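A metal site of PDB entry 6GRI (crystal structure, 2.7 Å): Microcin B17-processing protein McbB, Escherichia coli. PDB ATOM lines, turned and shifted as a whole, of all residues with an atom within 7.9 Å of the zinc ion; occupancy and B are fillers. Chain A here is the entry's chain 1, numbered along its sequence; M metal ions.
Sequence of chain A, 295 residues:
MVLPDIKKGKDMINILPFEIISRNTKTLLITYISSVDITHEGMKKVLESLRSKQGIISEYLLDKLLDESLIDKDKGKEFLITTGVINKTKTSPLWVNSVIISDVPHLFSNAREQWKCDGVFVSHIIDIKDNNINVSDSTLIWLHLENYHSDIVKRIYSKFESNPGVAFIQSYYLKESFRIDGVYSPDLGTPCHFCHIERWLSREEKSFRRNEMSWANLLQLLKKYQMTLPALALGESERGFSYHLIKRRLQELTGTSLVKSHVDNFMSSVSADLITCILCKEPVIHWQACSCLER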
ATOM      1  N   TYR A 157     -13.747   9.144 -21.067  1.00  0.00           N
ATOM      2  CA  TYR A 157     -14.397  10.029 -22.059  1.00  0.00           C
ATOM      3  C   TYR A 157     -13.590  10.057 -23.351  1.00  0.00           C
ATOM      4  O   TYR A 157     -14.134   9.906 -24.432  1.00  0.00           O
ATOM      5  CB  TYR A 157     -14.587  11.456 -21.492  1.00  0.00           C
ATOM      6  CG  TYR A 157     -15.739  11.651 -20.497  1.00  0.00           C
ATOM      7  CD1 TYR A 157     -16.539  10.578 -20.055  1.00  0.00           C
ATOM      8  CD2 TYR A 157     -16.003  12.914 -19.981  1.00  0.00           C
ATOM      9  CE1 TYR A 157     -17.558  10.772 -19.142  1.00  0.00           C
ATOM     10  CE2 TYR A 157     -17.022  13.111 -19.055  1.00  0.00           C
ATOM     11  CZ  TYR A 157     -17.800  12.038 -18.642  1.00  0.00           C
ATOM     12  OH  TYR A 157     -18.814  12.226 -17.736  1.00  0.00           O
ATOM     13  N   GLU A 161     -16.178   8.825 -25.833  1.00  0.00           N
ATOM     14  CA  GLU A 161     -17.052   9.975 -26.195  1.00  0.00           C
ATOM     15  C   GLU A 161     -17.618   9.981 -27.612  1.00  0.00           C
ATOM     16  O   GLU A 161     -18.742  10.469 -27.813  1.00  0.00           O
ATOM     17  CB  GLU A 161     -16.353  11.322 -25.962  1.00  0.00           C
ATOM     18  CG  GLU A 161     -16.610  11.913 -24.582  1.00  0.00           C
ATOM     19  CD  GLU A 161     -15.957  13.264 -24.392  1.00  0.00           C
ATOM     20  OE1 GLU A 161     -15.188  13.703 -25.286  1.00  0.00           O
ATOM     21  OE2 GLU A 161     -16.210  13.910 -23.343  1.00  0.00           O
ATOM     22  N   TYR A 184     -24.705  11.544 -19.064  1.00  0.00           N
ATOM     23  CA  TYR A 184     -23.943  12.320 -20.050  1.00  0.00           C
ATOM     24  C   TYR A 184     -24.129  11.653 -21.401  1.00  0.00           C
ATOM     25  O   TYR A 184     -23.487  10.665 -21.689  1.00  0.00           O
ATOM     26  CB  TYR A 184     -22.456  12.369 -19.660  1.00  0.00           C
ATOM     27  CG  TYR A 184     -21.545  12.958 -20.712  1.00  0.00           C
ATOM     28  CD1 TYR A 184     -21.921  14.064 -21.461  1.00  0.00           C
ATOM     29  CD2 TYR A 184     -20.286  12.395 -20.961  1.00  0.00           C
ATOM     30  CE1 TYR A 184     -21.086  14.586 -22.447  1.00  0.00           C
ATOM     31  CE2 TYR A 184     -19.439  12.924 -21.927  1.00  0.00           C
ATOM     32  CZ  TYR A 184     -19.856  14.016 -22.664  1.00  0.00           C
ATOM     33  OH  TYR A 184     -19.049  14.554 -23.624  1.00  0.00           O
ATOM     34  N   THR A 190     -26.312  16.555 -22.968  1.00  0.00           N
ATOM     35  CA  THR A 190     -26.473  16.710 -21.522  1.00  0.00           C
ATOM     36  C   THR A 190     -25.154  16.973 -20.797  1.00  0.00           C
ATOM     37  O   THR A 190     -24.092  16.658 -21.309  1.00  0.00           O
ATOM     38  CB  THR A 190     -27.137  15.476 -20.905  1.00  0.00           C
ATOM     39  OG1 THR A 190     -26.374  14.317 -21.233  1.00  0.00           O
ATOM     40  CG2 THR A 190     -28.562  15.308 -21.452  1.00  0.00           C
ATOM     41  N   PRO A 191     -25.213  17.575 -19.606  1.00  0.00           N
ATOM     42  CA  PRO A 191     -23.988  17.821 -18.846  1.00  0.00           C
ATOM     43  C   PRO A 191     -23.141  16.587 -18.538  1.00  0.00           C
ATOM     44  O   PRO A 191     -23.669  15.520 -18.199  1.00  0.00           O
ATOM     45  CB  PRO A 191     -24.517  18.427 -17.563  1.00  0.00           C
ATOM     46  CG  PRO A 191     -25.721  19.176 -17.991  1.00  0.00           C
ATOM     47  CD  PRO A 191     -26.352  18.333 -19.054  1.00  0.00           C
ATOM     48  N   CYS A 192     -21.830  16.758 -18.646  1.00  0.00           N
ATOM     49  CA  CYS A 192     -20.855  15.701 -18.372  1.00  0.00           C
ATOM     50  C   CYS A 192     -20.480  15.637 -16.880  1.00  0.00           C
ATOM     51  O   CYS A 192     -20.989  16.419 -16.098  1.00  0.00           O
ATOM     52  CB  CYS A 192     -19.593  15.952 -19.189  1.00  0.00           C
ATOM     53  SG  CYS A 192     -18.540  17.212 -18.456  1.00  0.00           S
ATOM     54  N   HIS A 193     -19.571  14.728 -16.512  1.00  0.00           N
ATOM     55  CA  HIS A 193     -19.098  14.607 -15.127  1.00  0.00           C
ATOM     56  C   HIS A 193     -18.615  15.915 -14.547  1.00  0.00           C
ATOM     57  O   HIS A 193     -18.875  16.198 -13.392  1.00  0.00           O
ATOM     58  CB  HIS A 193     -17.936  13.630 -15.019  1.00  0.00           C
ATOM     59  CG  HIS A 193     -17.284  13.614 -13.667  1.00  0.00           C
ATOM     60  ND1 HIS A 193     -17.996  13.389 -12.509  1.00  0.00           N
ATOM     61  CD2 HIS A 193     -16.003  13.812 -13.303  1.00  0.00           C
ATOM     62  CE1 HIS A 193     -17.162  13.421 -11.477  1.00  0.00           C
ATOM     63  NE2 HIS A 193     -15.949  13.679 -11.933  1.00  0.00           N
ATOM     64  N   PHE A 194     -17.882  16.679 -15.349  1.00  0.00           N
ATOM     65  CA  PHE A 194     -17.174  17.866 -14.837  1.00  0.00           C
ATOM     66  C   PHE A 194     -18.099  19.043 -14.581  1.00  0.00           C
ATOM     67  O   PHE A 194     -17.825  19.873 -13.707  1.00  0.00           O
ATOM     68  CB  PHE A 194     -16.012  18.233 -15.769  1.00  0.00           C
ATOM     69  CG  PHE A 194     -14.952  17.175 -15.815  1.00  0.00           C
ATOM     70  CD1 PHE A 194     -14.141  16.972 -14.718  1.00  0.00           C
ATOM     71  CD2 PHE A 194     -14.804  16.353 -16.912  1.00  0.00           C
ATOM     72  CE1 PHE A 194     -13.185  15.976 -14.716  1.00  0.00           C
ATOM     73  CE2 PHE A 194     -13.858  15.364 -16.926  1.00  0.00           C
ATOM     74  CZ  PHE A 194     -13.034  15.178 -15.818  1.00  0.00           C
ATOM     75  N   CYS A 195     -19.194  19.115 -15.346  1.00  0.00           N
ATOM     76  CA  CYS A 195     -20.305  19.997 -15.024  1.00  0.00           C
ATOM     77  C   CYS A 195     -20.923  19.700 -13.650  1.00  0.00           C
ATOM     78  O   CYS A 195     -21.325  20.618 -12.928  1.00  0.00           O
ATOM     79  CB  CYS A 195     -21.381  19.921 -16.120  1.00  0.00           C
ATOM     80  SG  CYS A 195     -20.888  20.662 -17.691  1.00  0.00           S
ATOM     81  N   HIS A 196     -21.008  18.423 -13.286  1.00  0.00           N
ATOM     82  CA  HIS A 196     -21.551  18.014 -11.986  1.00  0.00           C
ATOM     83  C   HIS A 196     -20.647  18.327 -10.826  1.00  0.00           C
ATOM     84  O   HIS A 196     -21.089  19.006  -9.887  1.00  0.00           O
ATOM     85  CB  HIS A 196     -21.896  16.531 -11.984  1.00  0.00           C
ATOM     86  CG  HIS A 196     -23.116  16.220 -12.774  1.00  0.00           C
ATOM     87  ND1 HIS A 196     -23.082  16.073 -14.139  1.00  0.00           N
ATOM     88  CD2 HIS A 196     -24.406  16.065 -12.402  1.00  0.00           C
ATOM     89  CE1 HIS A 196     -24.311  15.825 -14.573  1.00  0.00           C
ATOM     90  NE2 HIS A 196     -25.122  15.823 -13.539  1.00  0.00           N
ATOM     91  N   ILE A 285     -26.856  22.279 -14.469  1.00  0.00           N
ATOM     92  CA  ILE A 285     -26.523  23.013 -15.694  1.00  0.00           C
ATOM     93  C   ILE A 285     -25.097  22.743 -16.204  1.00  0.00           C
ATOM     94  O   ILE A 285     -24.208  22.305 -15.465  1.00  0.00           O
ATOM     95  CB  ILE A 285     -26.718  24.537 -15.538  1.00  0.00           C
ATOM     96  CG1 ILE A 285     -25.620  25.193 -14.665  1.00  0.00           C
ATOM     97  CG2 ILE A 285     -28.106  24.839 -14.978  1.00  0.00           C
ATOM     98  CD1 ILE A 285     -25.811  26.690 -14.497  1.00  0.00           C
ATOM     99  N   HIS A 286     -24.879  23.036 -17.486  1.00  0.00           N
ATOM    100  CA  HIS A 286     -23.528  23.066 -18.043  1.00  0.00           C
ATOM    101  C   HIS A 286     -22.671  24.103 -17.322  1.00  0.00           C
ATOM    102  O   HIS A 286     -23.089  25.247 -17.146  1.00  0.00           O
ATOM    103  CB  HIS A 286     -23.566  23.359 -19.541  1.00  0.00           C
ATOM    104  CG  HIS A 286     -24.176  22.248 -20.340  1.00  0.00           C
ATOM    105  ND1 HIS A 286     -25.437  22.326 -20.892  1.00  0.00           N
ATOM    106  CD2 HIS A 286     -23.704  21.013 -20.643  1.00  0.00           C
ATOM    107  CE1 HIS A 286     -25.710  21.200 -21.523  1.00  0.00           C
ATOM    108  NE2 HIS A 286     -24.678  20.375 -21.378  1.00  0.00           N
ATOM    109  N   TRP A 287     -21.511  23.663 -16.843  1.00  0.00           N
ATOM    110  CA  TRP A 287     -20.442  24.567 -16.354  1.00  0.00           C
ATOM    111  C   TRP A 287     -19.911  25.428 -17.503  1.00  0.00           C
ATOM    112  O   TRP A 287     -19.530  24.898 -18.558  1.00  0.00           O
ATOM    113  CB  TRP A 287     -19.315  23.730 -15.725  1.00  0.00           C
ATOM    114  CG  TRP A 287     -18.198  24.473 -15.102  1.00  0.00           C
ATOM    115  CD1 TRP A 287     -18.281  25.630 -14.410  1.00  0.00           C
ATOM    116  CD2 TRP A 287     -16.809  24.083 -15.051  1.00  0.00           C
ATOM    117  NE1 TRP A 287     -17.033  26.003 -13.951  1.00  0.00           N
ATOM    118  CE2 TRP A 287     -16.115  25.061 -14.328  1.00  0.00           C
ATOM    119  CE3 TRP A 287     -16.087  22.986 -15.557  1.00  0.00           C
ATOM    120  CZ2 TRP A 287     -14.744  25.000 -14.093  1.00  0.00           C
ATOM    121  CZ3 TRP A 287     -14.704  22.927 -15.329  1.00  0.00           C
ATOM    122  CH2 TRP A 287     -14.054  23.931 -14.604  1.00  0.00           C
ATOM    123  N   GLN A 288     -19.895  26.735 -17.300  1.00  0.00           N
ATOM    124  CA  GLN A 288     -19.420  27.660 -18.331  1.00  0.00           C
ATOM    125  C   GLN A 288     -18.022  27.296 -18.886  1.00  0.00           C
ATOM    126  O   GLN A 288     -17.794  27.393 -20.098  1.00  0.00           O
ATOM    127  CB  GLN A 288     -19.470  29.101 -17.808  1.00  0.00           C
ATOM    128  CG  GLN A 288     -18.557  29.397 -16.623  1.00  0.00           C
ATOM    129  CD  GLN A 288     -19.084  30.501 -15.698  1.00  0.00           C
ATOM    130  OE1 GLN A 288     -19.965  31.289 -16.070  1.00  0.00           O
ATOM    131  NE2 GLN A 288     -18.525  30.558 -14.497  1.00  0.00           N
ATOM    132  N   ALA A 289     -17.127  26.843 -18.013  1.00  0.00           N
ATOM    133  CA  ALA A 289     -15.765  26.499 -18.391  1.00  0.00           C
ATOM    134  C   ALA A 289     -15.589  25.111 -19.022  1.00  0.00           C
ATOM    135  O   ALA A 289     -14.602  24.876 -19.709  1.00  0.00           O
ATOM    136  CB  ALA A 289     -14.820  26.647 -17.197  1.00  0.00           C
ATOM    137  N   CYS A 290     -16.521  24.198 -18.798  1.00  0.00           N
ATOM    138  CA  CYS A 290     -16.423  22.829 -19.352  1.00  0.00           C
ATOM    139  C   CYS A 290     -16.516  22.813 -20.871  1.00  0.00           C
ATOM    140  O   CYS A 290     -17.148  23.669 -21.460  1.00  0.00           O
ATOM    141  CB  CYS A 290     -17.550  21.974 -18.809  1.00  0.00           C
ATOM    142  SG  CYS A 290     -17.321  20.211 -19.046  1.00  0.00           S
ATOM    143  N   SER A 291     -15.924  21.808 -21.479  1.00  0.00           N
ATOM    144  CA  SER A 291     -15.880  21.710 -22.949  1.00  0.00           C
ATOM    145  C   SER A 291     -16.798  20.633 -23.550  1.00  0.00           C
ATOM    146  O   SER A 291     -16.850  20.487 -24.776  1.00  0.00           O
ATOM    147  CB  SER A 291     -14.437  21.483 -23.389  1.00  0.00           C
ATOM    148  OG  SER A 291     -13.852  20.442 -22.609  1.00  0.00           O
ATOM    149  N   CYS A 292     -17.545  19.901 -22.726  1.00  0.00           N
ATOM    150  CA  CYS A 292     -18.436  18.852 -23.219  1.00  0.00           C
ATOM    151  C   CYS A 292     -19.383  19.270 -24.379  1.00  0.00           C
ATOM    152  O   CYS A 292     -19.714  18.447 -25.209  1.00  0.00           O
ATOM    153  CB  CYS A 292     -19.236  18.204 -22.063  1.00  0.00           C
ATOM    154  SG  CYS A 292     -20.330  19.276 -21.095  1.00  0.00           S
ATOM    155  N   LEU A 293     -19.808  20.531 -24.422  1.00  0.00           N
ATOM    156  CA  LEU A 293     -20.711  21.029 -25.477  1.00  0.00           C
ATOM    157  C   LEU A 293     -19.974  21.235 -26.791  1.00  0.00           C
ATOM    158  O   LEU A 293     -20.549  21.061 -27.859  1.00  0.00           O
ATOM    159  CB  LEU A 293     -21.352  22.366 -25.089  1.00  0.00           C
ATOM    160  CG  LEU A 293     -22.079  22.441 -23.748  1.00  0.00           C
ATOM    161  CD1 LEU A 293     -21.271  23.194 -22.692  1.00  0.00           C
ATOM    162  CD2 LEU A 293     -23.429  23.104 -23.937  1.00  0.00           C
ATOM    163  N   ARG A 295     -17.375  19.623 -27.905  1.00  0.00           N
ATOM    164  CA  ARG A 295     -16.995  18.357 -28.517  1.00  0.00           C
ATOM    165  C   ARG A 295     -18.155  17.770 -29.331  1.00  0.00           C
ATOM    166  O   ARG A 295     -19.325  18.071 -29.109  1.00  0.00           O
ATOM    167  CB  ARG A 295     -16.478  17.360 -27.463  1.00  0.00           C
ATOM    168  CG  ARG A 295     -15.128  17.768 -26.870  1.00  0.00           C
ATOM    169  CD  ARG A 295     -14.225  16.616 -26.465  1.00  0.00           C
ATOM    170  NE  ARG A 295     -14.053  16.504 -25.015  1.00  0.00           N
ATOM    171  CZ  ARG A 295     -13.178  17.193 -24.266  1.00  0.00           C
ATOM    172  NH1 ARG A 295     -12.348  18.097 -24.797  1.00  0.00           N
ATOM    173  NH2 ARG A 295     -13.144  16.983 -22.951  1.00  0.00           N
ATOM    174  OXT ARG A 295     -17.931  17.000 -30.267  1.00  0.00           O
HETATM  175 ZN    ZN M   1     -19.445  19.281 -18.944  1.00  0.00          ZN
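Within 4 Å of the zinc ion: Cys 192, Cys 195, Cys 290 and Cys 292.
SG of Cys 192 sits close to N of Phe 194. The backbone carbonyl oxygen (O) of Cys 192 sits at hydrogen-bond distance from a ring nitrogen (ND1) of His 196, at 2.9 Å. SG of Cys 195 sits close to N of Trp 287, 3.2 Å away.
The zinc ion is bound by SG of Cys 192 (2.3 Å), SG of Cys 290 (2.3 Å), SG of Cys 292 (2.3 Å) and SG of Cys 195 (2.4 Å). The zinc ion has four donor atoms within binding distance.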
